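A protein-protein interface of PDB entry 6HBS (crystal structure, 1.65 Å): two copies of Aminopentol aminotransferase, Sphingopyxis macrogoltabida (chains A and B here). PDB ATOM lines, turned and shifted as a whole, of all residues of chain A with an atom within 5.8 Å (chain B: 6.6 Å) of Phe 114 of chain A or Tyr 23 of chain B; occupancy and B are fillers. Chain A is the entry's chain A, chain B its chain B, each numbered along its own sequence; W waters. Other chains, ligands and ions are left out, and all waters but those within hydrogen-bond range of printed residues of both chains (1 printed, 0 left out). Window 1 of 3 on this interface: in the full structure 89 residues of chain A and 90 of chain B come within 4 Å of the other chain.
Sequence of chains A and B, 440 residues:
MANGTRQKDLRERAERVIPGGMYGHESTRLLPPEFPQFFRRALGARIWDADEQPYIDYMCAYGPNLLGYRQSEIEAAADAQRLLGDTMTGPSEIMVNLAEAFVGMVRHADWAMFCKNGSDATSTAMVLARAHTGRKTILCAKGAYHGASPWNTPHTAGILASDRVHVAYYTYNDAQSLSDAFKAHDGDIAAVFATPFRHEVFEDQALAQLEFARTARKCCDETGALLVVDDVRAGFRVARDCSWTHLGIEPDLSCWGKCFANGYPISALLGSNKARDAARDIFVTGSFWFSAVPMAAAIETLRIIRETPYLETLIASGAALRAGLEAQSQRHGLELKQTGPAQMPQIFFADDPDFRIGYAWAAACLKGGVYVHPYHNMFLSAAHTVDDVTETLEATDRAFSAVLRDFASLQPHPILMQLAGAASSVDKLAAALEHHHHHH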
ATOM      1  N   MET A  95       1.926   2.476   4.773  1.00  0.00           N
ATOM      2  CA  MET A  95       2.187   2.135   3.361  1.00  0.00           C
ATOM      3  C   MET A  95       3.245   1.028   3.257  1.00  0.00           C
ATOM      4  O   MET A  95       3.105   0.105   2.437  1.00  0.00           O
ATOM      5  CB  MET A  95       2.628   3.341   2.529  1.00  0.00           C
ATOM      6  CG  MET A  95       2.718   3.034   1.033  1.00  0.00           C
ATOM      7  SD  MET A  95       3.236   4.474   0.086  1.00  0.00           S
ATOM      8  CE  MET A  95       3.209   3.794  -1.574  1.00  0.00           C
ATOM      9  N   LEU A  98       1.665  -2.258   4.401  1.00  0.00           N
ATOM     10  CA  LEU A  98       0.757  -2.777   3.367  1.00  0.00           C
ATOM     11  C   LEU A  98       1.566  -3.416   2.226  1.00  0.00           C
ATOM     12  O   LEU A  98       1.241  -4.532   1.813  1.00  0.00           O
ATOM     13  CB  LEU A  98      -0.158  -1.665   2.860  1.00  0.00           C
ATOM     14  CG  LEU A  98      -1.029  -2.025   1.665  1.00  0.00           C
ATOM     15  CD1 LEU A  98      -1.989  -3.158   1.993  1.00  0.00           C
ATOM     16  CD2 LEU A  98      -1.749  -0.801   1.168  1.00  0.00           C
ATOM     17  N   ALA A  99       2.616  -2.746   1.743  1.00  0.00           N
ATOM     18  CA  ALA A  99       3.408  -3.284   0.652  1.00  0.00           C
ATOM     19  C   ALA A  99       4.054  -4.601   1.082  1.00  0.00           C
ATOM     20  O   ALA A  99       4.093  -5.541   0.298  1.00  0.00           O
ATOM     21  CB  ALA A  99       4.430  -2.298   0.175  1.00  0.00           C
ATOM     22  N   PHE A 102       1.236  -7.308   1.104  1.00  0.00           N
ATOM     23  CA  PHE A 102       0.709  -7.684  -0.205  1.00  0.00           C
ATOM     24  C   PHE A 102       1.785  -8.468  -0.970  1.00  0.00           C
ATOM     25  O   PHE A 102       1.495  -9.494  -1.544  1.00  0.00           O
ATOM     26  CB  PHE A 102       0.183  -6.450  -0.941  1.00  0.00           C
ATOM     27  CG  PHE A 102      -0.993  -6.672  -1.861  1.00  0.00           C
ATOM     28  CD1 PHE A 102      -1.111  -7.829  -2.632  1.00  0.00           C
ATOM     29  CD2 PHE A 102      -1.954  -5.689  -2.008  1.00  0.00           C
ATOM     30  CE1 PHE A 102      -2.197  -8.014  -3.476  1.00  0.00           C
ATOM     31  CE2 PHE A 102      -3.026  -5.863  -2.877  1.00  0.00           C
ATOM     32  CZ  PHE A 102      -3.137  -7.020  -3.617  1.00  0.00           C
ATOM     33  N   ALA A 112       5.208  -3.616  -4.728  1.00  0.00           N
ATOM     34  CA  ALA A 112       3.860  -3.123  -4.974  1.00  0.00           C
ATOM     35  C   ALA A 112       3.855  -1.606  -5.225  1.00  0.00           C
ATOM     36  O   ALA A 112       4.635  -0.880  -4.651  1.00  0.00           O
ATOM     37  CB  ALA A 112       2.999  -3.481  -3.805  1.00  0.00           C
ATOM     38  N   MET A 113       2.908  -1.153  -6.053  1.00  0.00           N
ATOM     39  CA  MET A 113       2.555   0.237  -6.187  1.00  0.00           C
ATOM     40  C   MET A 113       1.040   0.363  -5.967  1.00  0.00           C
ATOM     41  O   MET A 113       0.281  -0.541  -6.392  1.00  0.00           O
ATOM     42  CB  MET A 113       2.954   0.772  -7.568  1.00  0.00           C
ATOM     43  CG  MET A 113       4.457   0.716  -7.805  1.00  0.00           C
ATOM     44  SD  MET A 113       4.897   1.148  -9.502  1.00  0.00           S
ATOM     45  CE  MET A 113       4.673   2.922  -9.491  1.00  0.00           C
ATOM     46  N   PHE A 114       0.610   1.431  -5.262  1.00  0.00           N
ATOM     47  CA  PHE A 114      -0.779   1.639  -4.905  1.00  0.00           C
ATOM     48  C   PHE A 114      -1.298   2.858  -5.644  1.00  0.00           C
ATOM     49  O   PHE A 114      -0.578   3.879  -5.767  1.00  0.00           O
ATOM     50  CB  PHE A 114      -0.947   1.743  -3.380  1.00  0.00           C
ATOM     51  CG  PHE A 114      -0.506   0.480  -2.681  1.00  0.00           C
ATOM     52  CD1 PHE A 114      -1.222  -0.692  -2.842  1.00  0.00           C
ATOM     53  CD2 PHE A 114       0.671   0.437  -1.954  1.00  0.00           C
ATOM     54  CE1 PHE A 114      -0.772  -1.879  -2.290  1.00  0.00           C
ATOM     55  CE2 PHE A 114       1.134  -0.761  -1.429  1.00  0.00           C
ATOM     56  CZ  PHE A 114       0.420  -1.914  -1.607  1.00  0.00           C
ATOM     57  N   CYS A 115      -2.554   2.749  -6.087  1.00  0.00           N
ATOM     58  CA  CYS A 115      -3.285   3.782  -6.833  1.00  0.00           C
ATOM     59  C   CYS A 115      -4.756   3.756  -6.394  1.00  0.00           C
ATOM     60  O   CYS A 115      -5.064   3.219  -5.322  1.00  0.00           O
ATOM     61  CB  CYS A 115      -3.108   3.557  -8.333  1.00  0.00           C
ATOM     62  SG  CYS A 115      -3.383   1.824  -8.800  1.00  0.00           S
ATOM     63  N   LYS A 116      -5.658   4.384  -7.159  1.00  0.00           N
ATOM     64  CA  LYS A 116      -7.054   4.433  -6.748  1.00  0.00           C
ATOM     65  C   LYS A 116      -7.905   3.433  -7.532  1.00  0.00           C
ATOM     66  O   LYS A 116      -8.584   2.620  -6.928  1.00  0.00           O
ATOM     67  CB  LYS A 116      -7.642   5.834  -6.897  1.00  0.00           C
ATOM     68  CG  LYS A 116      -7.222   6.812  -5.815  1.00  0.00           C
ATOM     69  CD  LYS A 116      -7.726   6.494  -4.411  1.00  0.00           C
ATOM     70  CE  LYS A 116      -6.633   5.973  -3.513  1.00  0.00           C
ATOM     71  NZ  LYS A 116      -7.061   5.969  -2.109  1.00  0.00           N
ATOM     72  N   PHE A 260      -9.868  -5.607  -2.216  1.00  0.00           N
ATOM     73  CA  PHE A 260      -8.805  -5.931  -1.213  1.00  0.00           C
ATOM     74  C   PHE A 260      -8.771  -4.959  -0.017  1.00  0.00           C
ATOM     75  O   PHE A 260      -7.991  -5.158   0.912  1.00  0.00           O
ATOM     76  CB  PHE A 260      -7.437  -6.160  -1.844  1.00  0.00           C
ATOM     77  CG  PHE A 260      -6.693  -4.976  -2.393  1.00  0.00           C
ATOM     78  CD1 PHE A 260      -6.019  -4.101  -1.555  1.00  0.00           C
ATOM     79  CD2 PHE A 260      -6.607  -4.777  -3.760  1.00  0.00           C
ATOM     80  CE1 PHE A 260      -5.325  -3.023  -2.081  1.00  0.00           C
ATOM     81  CE2 PHE A 260      -5.899  -3.707  -4.281  1.00  0.00           C
ATOM     82  CZ  PHE A 260      -5.238  -2.840  -3.446  1.00  0.00           C
ATOM     83  N   ILE A 266      -8.863   1.669  -3.238  1.00  0.00           N
ATOM     84  CA  ILE A 266      -7.461   1.435  -3.395  1.00  0.00           C
ATOM     85  C   ILE A 266      -7.295   0.281  -4.407  1.00  0.00           C
ATOM     86  O   ILE A 266      -8.075  -0.683  -4.416  1.00  0.00           O
ATOM     87  CB  ILE A 266      -6.749   1.148  -2.064  1.00  0.00           C
ATOM     88  CG1 ILE A 266      -5.247   0.939  -2.261  1.00  0.00           C
ATOM     89  CG2 ILE A 266      -7.384  -0.023  -1.309  1.00  0.00           C
ATOM     90  CD1 ILE A 266      -4.440   1.029  -0.994  1.00  0.00           C
ATOM     91  N   SER A 267      -6.276   0.424  -5.247  1.00  0.00           N
ATOM     92  CA  SER A 267      -5.901  -0.561  -6.308  1.00  0.00           C
ATOM     93  C   SER A 267      -4.389  -0.703  -6.266  1.00  0.00           C
ATOM     94  O   SER A 267      -3.701   0.077  -5.582  1.00  0.00           O
ATOM     95  CB  SER A 267      -6.418  -0.135  -7.683  1.00  0.00           C
ATOM     96  OG  SER A 267      -7.845  -0.034  -7.690  1.00  0.00           O
ATOM     97  N   ALA A 268      -3.854  -1.731  -6.928  1.00  0.00           N
ATOM     98  CA  ALA A 268      -2.452  -2.042  -6.805  1.00  0.00           C
ATOM     99  C   ALA A 268      -1.920  -2.664  -8.087  1.00  0.00           C
ATOM    100  O   ALA A 268      -2.624  -3.438  -8.748  1.00  0.00           O
ATOM    101  CB  ALA A 268      -2.199  -3.002  -5.672  1.00  0.00           C
ATOM    102  N   LEU A 269      -0.645  -2.370  -8.340  1.00  0.00           N
ATOM    103  CA  LEU A 269       0.214  -3.114  -9.266  1.00  0.00           C
ATOM    104  C   LEU A 269       1.272  -3.895  -8.477  1.00  0.00           C
ATOM    105  O   LEU A 269       2.073  -3.302  -7.759  1.00  0.00           O
ATOM    106  CB  LEU A 269       0.856  -2.132 -10.244  1.00  0.00           C
ATOM    107  CG  LEU A 269       1.721  -2.798 -11.327  1.00  0.00           C
ATOM    108  CD1 LEU A 269       0.878  -3.759 -12.137  1.00  0.00           C
ATOM    109  CD2 LEU A 269       2.353  -1.763 -12.248  1.00  0.00           C
ATOM    110  N   LEU A 270       1.285  -5.222  -8.621  1.00  0.00           N
ATOM    111  CA  LEU A 270       2.278  -6.136  -7.992  1.00  0.00           C
ATOM    112  C   LEU A 270       3.243  -6.613  -9.077  1.00  0.00           C
ATOM    113  O   LEU A 270       2.801  -6.923 -10.180  1.00  0.00           O
ATOM    114  CB  LEU A 270       1.558  -7.315  -7.341  1.00  0.00           C
ATOM    115  CG  LEU A 270       1.000  -7.116  -5.922  1.00  0.00           C
ATOM    116  CD1 LEU A 270       2.087  -7.197  -4.868  1.00  0.00           C
ATOM    117  CD2 LEU A 270       0.271  -5.793  -5.808  1.00  0.00           C
ATOM    118  N   ALA A 279       9.539   0.231 -13.432  1.00  0.00           N
ATOM    119  CA  ALA A 279       8.592   0.797 -12.491  1.00  0.00           C
ATOM    120  C   ALA A 279       9.135   2.106 -11.908  1.00  0.00           C
ATOM    121  O   ALA A 279       8.361   3.028 -11.619  1.00  0.00           O
ATOM    122  CB  ALA A 279       8.318  -0.188 -11.387  1.00  0.00           C
ATOM    123  N   VAL A 284       4.023   7.936 -12.639  1.00  0.00           N
ATOM    124  CA  VAL A 284       2.622   7.708 -12.360  1.00  0.00           C
ATOM    125  C   VAL A 284       2.384   8.199 -10.924  1.00  0.00           C
ATOM    126  O   VAL A 284       3.221   8.014 -10.038  1.00  0.00           O
ATOM    127  CB  VAL A 284       2.227   6.235 -12.573  1.00  0.00           C
ATOM    128  CG1 VAL A 284       2.424   5.779 -14.019  1.00  0.00           C
ATOM    129  CG2 VAL A 284       2.957   5.305 -11.614  1.00  0.00           C
ATOM    130  N   THR A 285       1.276   8.906 -10.726  1.00  0.00           N
ATOM    131  CA  THR A 285       0.947   9.436  -9.404  1.00  0.00           C
ATOM    132  C   THR A 285      -0.527   9.818  -9.386  1.00  0.00           C
ATOM    133  O   THR A 285      -1.161   9.934 -10.443  1.00  0.00           O
ATOM    134  CB  THR A 285       1.827  10.657  -9.100  1.00  0.00           C
ATOM    135  OG1 THR A 285       1.869  10.913  -7.693  1.00  0.00           O
ATOM    136  CG2 THR A 285       1.394  11.898  -9.864  1.00  0.00           C
ATOM    137  N   TRP A 289      -3.390   8.833  -4.007  1.00  0.00           N
ATOM    138  CA  TRP A 289      -2.773   7.491  -4.081  1.00  0.00           C
ATOM    139  C   TRP A 289      -2.040   7.120  -2.795  1.00  0.00           C
ATOM    140  O   TRP A 289      -1.718   5.941  -2.619  1.00  0.00           O
ATOM    141  CB  TRP A 289      -1.834   7.373  -5.293  1.00  0.00           C
ATOM    142  CG  TRP A 289      -2.520   7.392  -6.633  1.00  0.00           C
ATOM    143  CD1 TRP A 289      -3.771   7.860  -6.935  1.00  0.00           C
ATOM    144  CD2 TRP A 289      -1.968   6.923  -7.884  1.00  0.00           C
ATOM    145  NE1 TRP A 289      -4.039   7.682  -8.274  1.00  0.00           N
ATOM    146  CE2 TRP A 289      -2.946   7.132  -8.879  1.00  0.00           C
ATOM    147  CE3 TRP A 289      -0.757   6.334  -8.246  1.00  0.00           C
ATOM    148  CZ2 TRP A 289      -2.720   6.819 -10.228  1.00  0.00           C
ATOM    149  CZ3 TRP A 289      -0.536   6.017  -9.575  1.00  0.00           C
ATOM    150  CH2 TRP A 289      -1.524   6.223 -10.536  1.00  0.00           C
ATOM    151  N   PHE A 290      -1.720   8.110  -1.942  1.00  0.00           N
ATOM    152  CA  PHE A 290      -0.886   7.912  -0.769  1.00  0.00           C
ATOM    153  C   PHE A 290      -1.723   7.995   0.516  1.00  0.00           C
ATOM    154  O   PHE A 290      -1.156   8.019   1.613  1.00  0.00           O
ATOM    155  CB  PHE A 290       0.290   8.901  -0.791  1.00  0.00           C
ATOM    156  CG  PHE A 290       1.053   8.809  -2.093  1.00  0.00           C
ATOM    157  CD1 PHE A 290       1.848   7.714  -2.349  1.00  0.00           C
ATOM    158  CD2 PHE A 290       0.839   9.716  -3.107  1.00  0.00           C
ATOM    159  CE1 PHE A 290       2.479   7.566  -3.576  1.00  0.00           C
ATOM    160  CE2 PHE A 290       1.486   9.580  -4.325  1.00  0.00           C
ATOM    161  CZ  PHE A 290       2.312   8.509  -4.554  1.00  0.00           C
ATOM    162  N   MET A 295      -5.433   2.286   3.021  1.00  0.00           N
ATOM    163  CA  MET A 295      -4.357   1.371   3.245  1.00  0.00           C
ATOM    164  C   MET A 295      -4.558   0.577   4.548  1.00  0.00           C
ATOM    165  O   MET A 295      -4.222  -0.640   4.605  1.00  0.00           O
ATOM    166  CB  MET A 295      -3.013   2.088   3.261  1.00  0.00           C
ATOM    167  CG  MET A 295      -2.644   2.650   1.897  1.00  0.00           C
ATOM    168  SD  MET A 295      -0.976   3.272   1.929  1.00  0.00           S
ATOM    169  CE  MET A 295      -1.002   4.175   0.388  1.00  0.00           C
ATOM    170  N   VAL B  17      10.187  -3.222  -0.961  1.00  0.00           N
ATOM    171  CA  VAL B  17       8.856  -3.689  -1.378  1.00  0.00           C
ATOM    172  C   VAL B  17       8.116  -2.633  -2.198  1.00  0.00           C
ATOM    173  O   VAL B  17       6.995  -2.902  -2.641  1.00  0.00           O
ATOM    174  CB  VAL B  17       8.011  -4.179  -0.193  1.00  0.00           C
ATOM    175  CG1 VAL B  17       8.611  -5.435   0.417  1.00  0.00           C
ATOM    176  CG2 VAL B  17       7.812  -3.105   0.842  1.00  0.00           C
ATOM    177  N   ILE B  18       8.729  -1.460  -2.394  1.00  0.00           N
ATOM    178  CA  ILE B  18       8.175  -0.414  -3.237  1.00  0.00           C
ATOM    179  C   ILE B  18       9.272   0.030  -4.197  1.00  0.00           C
ATOM    180  O   ILE B  18      10.395   0.271  -3.770  1.00  0.00           O
ATOM    181  CB  ILE B  18       7.641   0.754  -2.386  1.00  0.00           C
ATOM    182  CG1 ILE B  18       6.615   0.286  -1.360  1.00  0.00           C
ATOM    183  CG2 ILE B  18       7.098   1.870  -3.269  1.00  0.00           C
ATOM    184  CD1 ILE B  18       6.304   1.321  -0.287  1.00  0.00           C
ATOM    185  N   PRO B  19       9.012   0.181  -5.515  1.00  0.00           N
ATOM    186  CA  PRO B  19      10.072   0.565  -6.449  1.00  0.00           C
ATOM    187  C   PRO B  19      10.624   1.959  -6.083  1.00  0.00           C
ATOM    188  O   PRO B  19       9.863   2.934  -6.023  1.00  0.00           O
ATOM    189  CB  PRO B  19       9.396   0.577  -7.829  1.00  0.00           C
ATOM    190  CG  PRO B  19       8.122  -0.227  -7.623  1.00  0.00           C
ATOM    191  CD  PRO B  19       7.715   0.024  -6.184  1.00  0.00           C
ATOM    192  N   GLY B  20      11.933   2.005  -5.804  1.00  0.00           N
ATOM    193  CA  GLY B  20      12.668   3.214  -5.325  1.00  0.00           C
ATOM    194  C   GLY B  20      12.303   3.621  -3.891  1.00  0.00           C
ATOM    195  O   GLY B  20      12.708   4.680  -3.437  1.00  0.00           O
ATOM    196  N   GLY B  21      11.503   2.800  -3.201  1.00  0.00           N
ATOM    197  CA  GLY B  21      10.990   3.037  -1.838  1.00  0.00           C
ATOM    198  C   GLY B  21       9.813   4.000  -1.796  1.00  0.00           C
ATOM    199  O   GLY B  21       9.179   4.169  -0.759  1.00  0.00           O
ATOM    200  N   MET B  22       9.525   4.643  -2.926  1.00  0.00           N
ATOM    201  CA  MET B  22       8.384   5.551  -3.115  1.00  0.00           C
ATOM    202  C   MET B  22       8.422   6.092  -4.554  1.00  0.00           C
ATOM    203  O   MET B  22       9.352   5.832  -5.273  1.00  0.00           O
ATOM    204  CB  MET B  22       8.365   6.704  -2.096  1.00  0.00           C
ATOM    205  CG  MET B  22       7.199   6.573  -1.107  1.00  0.00           C
ATOM    206  SD  MET B  22       5.556   6.877  -1.852  1.00  0.00           S
ATOM    207  CE  MET B  22       5.616   8.659  -2.060  1.00  0.00           C
ATOM    208  N   TYR B  23       7.367   6.807  -4.963  1.00  0.00           N
ATOM    209  CA  TYR B  23       7.137   7.170  -6.385  1.00  0.00           C
ATOM    210  C   TYR B  23       6.152   8.341  -6.405  1.00  0.00           C
ATOM    211  O   TYR B  23       5.560   8.671  -5.363  1.00  0.00           O
ATOM    212  CB  TYR B  23       6.624   5.967  -7.190  1.00  0.00           C
ATOM    213  CG  TYR B  23       5.348   5.381  -6.628  1.00  0.00           C
ATOM    214  CD1 TYR B  23       4.102   5.862  -7.009  1.00  0.00           C
ATOM    215  CD2 TYR B  23       5.390   4.357  -5.695  1.00  0.00           C
ATOM    216  CE1 TYR B  23       2.934   5.352  -6.456  1.00  0.00           C
ATOM    217  CE2 TYR B  23       4.233   3.828  -5.144  1.00  0.00           C
ATOM    218  CZ  TYR B  23       3.007   4.333  -5.517  1.00  0.00           C
ATOM    219  OH  TYR B  23       1.888   3.836  -4.933  1.00  0.00           O
ATOM    220  N   GLY B  24       6.019   9.001  -7.558  1.00  0.00           N
ATOM    221  CA  GLY B  24       5.023  10.050  -7.742  1.00  0.00           C
ATOM    222  C   GLY B  24       5.398  11.374  -7.089  1.00  0.00           C
ATOM    223  O   GLY B  24       6.537  11.566  -6.692  1.00  0.00           O
ATOM    224  N   HIS B  25       4.412  12.279  -6.987  1.00  0.00           N
ATOM    225  CA  HIS B  25       4.597  13.677  -6.552  1.00  0.00           C
ATOM    226  C   HIS B  25       5.120  13.730  -5.103  1.00  0.00           C
ATOM    227  O   HIS B  25       5.845  14.671  -4.763  1.00  0.00           O
ATOM    228  CB  HIS B  25       3.300  14.520  -6.706  1.00  0.00           C
ATOM    229  CG  HIS B  25       3.344  15.603  -7.749  1.00  0.00           C
ATOM    230  ND1 HIS B  25       4.525  16.233  -8.150  1.00  0.00           N
ATOM    231  CD2 HIS B  25       2.350  16.211  -8.447  1.00  0.00           C
ATOM    232  CE1 HIS B  25       4.255  17.139  -9.075  1.00  0.00           C
ATOM    233  NE2 HIS B  25       2.928  17.150  -9.273  1.00  0.00           N
ATOM    234  N   GLU B  26       4.742  12.755  -4.256  1.00  0.00           N
ATOM    235  CA  GLU B  26       5.056  12.818  -2.805  1.00  0.00           C
ATOM    236  C   GLU B  26       6.396  12.140  -2.466  1.00  0.00           C
ATOM    237  O   GLU B  26       6.826  12.160  -1.297  1.00  0.00           O
ATOM    238  CB  GLU B  26       3.890  12.243  -1.990  1.00  0.00           C
ATOM    239  CG  GLU B  26       2.626  13.069  -2.153  1.00  0.00           C
ATOM    240  CD  GLU B  26       1.475  12.755  -1.207  1.00  0.00           C
ATOM    241  OE1 GLU B  26       1.652  11.951  -0.216  1.00  0.00           O
ATOM    242  OE2 GLU B  26       0.385  13.326  -1.457  1.00  0.00           O
ATOM    243  N   SER B  27       7.068  11.558  -3.465  1.00  0.00           N
ATOM    244  CA  SER B  27       8.418  11.074  -3.263  1.00  0.00           C
ATOM    245  C   SER B  27       9.323  12.251  -2.848  1.00  0.00           C
ATOM    246  O   SER B  27       9.236  13.351  -3.425  1.00  0.00           O
ATOM    247  CB  SER B  27       8.943  10.408  -4.512  1.00  0.00           C
ATOM    248  OG  SER B  27      10.294  10.033  -4.341  1.00  0.00           O
ATOM    249  N   GLN B  37       9.949  11.062   4.597  1.00  0.00           N
ATOM    250  CA  GLN B  37       9.103  10.459   3.545  1.00  0.00           C
ATOM    251  C   GLN B  37       7.785   9.986   4.155  1.00  0.00           C
ATOM    252  O   GLN B  37       6.732  10.130   3.534  1.00  0.00           O
ATOM    253  CB  GLN B  37       9.832   9.284   2.876  1.00  0.00           C
ATOM    254  CG  GLN B  37       9.040   8.610   1.752  1.00  0.00           C
ATOM    255  CD  GLN B  37       8.749   9.495   0.561  1.00  0.00           C
ATOM    256  OE1 GLN B  37       9.471   9.468  -0.452  1.00  0.00           O
ATOM    257  NE2 GLN B  37       7.659  10.246   0.654  1.00  0.00           N
HETATM  258  O   HOH W   1       6.078   7.541 -10.339  1.00  0.00           O
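The backbone NH (N) of Ala 112 of chain A lies within hydrogen-bond range of the backbone carbonyl oxygen (O) of Val 17 of chain B (2.8 Å).
O of Phe 114 of chain A lies within hydrogen-bond range of OH of Tyr 23 of chain B.
The side-chain hydroxyl (OG1) of Thr 285 of chain A lies within hydrogen-bond range of the backbone NH (N) of His 25 of chain B, 3.0 Å away.
N of Leu 269 of chain A lies within hydrogen-bond range of O of Met 113 of chain A.
The backbone carbonyl oxygen (O) of Glu 26 of chain B sits at hydrogen-bond distance from the side-chain amide nitrogen (NE2) of Gln 37 of chain B, at 2.9 Å.
Met 22 of chain B touches Met 95 of chain A (SD to SD, 3.9 Å).
Met 95 of chain A touches Tyr 23 of chain B.
Val 17 of chain B touches Ala 99 of chain A (CG2 to CB, 3.5 Å).
Ile 18 of chain B touches Ala 112 of chain A (CA to O, 3.8 Å).
Ala 112 of chain A touches Pro 19 of chain B (O to CD, 3.6 Å).
Met 113 of chain A touches Pro 19 of chain B (CG to CD, 3.7 Å).
Thr 285 of chain A touches Gly 24 of chain B (OG1 to CA, 3.3 Å).
Met 22 of chain B touches Phe 290 of chain A.
O of Tyr 23 of chain B touches CZ of Phe 290 of chain A (3.4 Å).
Glu 26 of chain B touches Phe 290 of chain A (OE1 to CB, 3.4 Å).
Phe 114 of chain A touches just one residue of chain B: Tyr 23 (2.6 Å).
Tyr 23 of chain B touches just these residues of chain A: Met 95, Met 113, Phe 114, Val 284 and Phe 290.
Of the printed residues of chain B, Ala 279 of chain A touches Pro 19 (3.8 Å).
Of the printed residues of chain A, Glu 26 of chain B touches Phe 290 (3.4 Å).
Printed residues of chain B within 4 Å of Ala 112 of chain A: Val 17, Ile 18 and Pro 19.
Of the printed residues of chain B, Met 113 of chain A touches Pro 19 (3.7 Å) and Tyr 23 (3.7 Å).
Printed residues of chain B within 4 Å of Phe 290 of chain A: Met 22, Tyr 23 and Glu 26.
Of the 12 printed residues of chain B, 8 touch a printed residue of chain A.
Hydrophobic or aromatic side chains of chain B that line the printed part of chain A: Val 17, Ile 18, Pro 19, Met 22 and Tyr 23.
Printed residues of chain A that touch a printed residue of chain B: Met 95, Ala 99, Ala 112, Met 113, Phe 114, Ala 279, Val 284, Thr 285 and Phe 290.
Hydrophobic or aromatic side chains of chain A that line the printed part of chain B: Met 95, Ala 99, Met 113, Phe 114, Ala 279 and Phe 290.
Among the printed residues, 18 pairs touch across the chains.
Among the printed residues, no Asp or Glu carboxylate lies within 4 Å of a Lys or Arg side-chain nitrogen of the other chain.
No position is printed for both chains.
Water W1 bridges the backbone carbonyl oxygen (O) of Val 284 of chain A (2.9 Å) and the backbone NH (N) of Gly 24 of chain B (3.1 Å).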
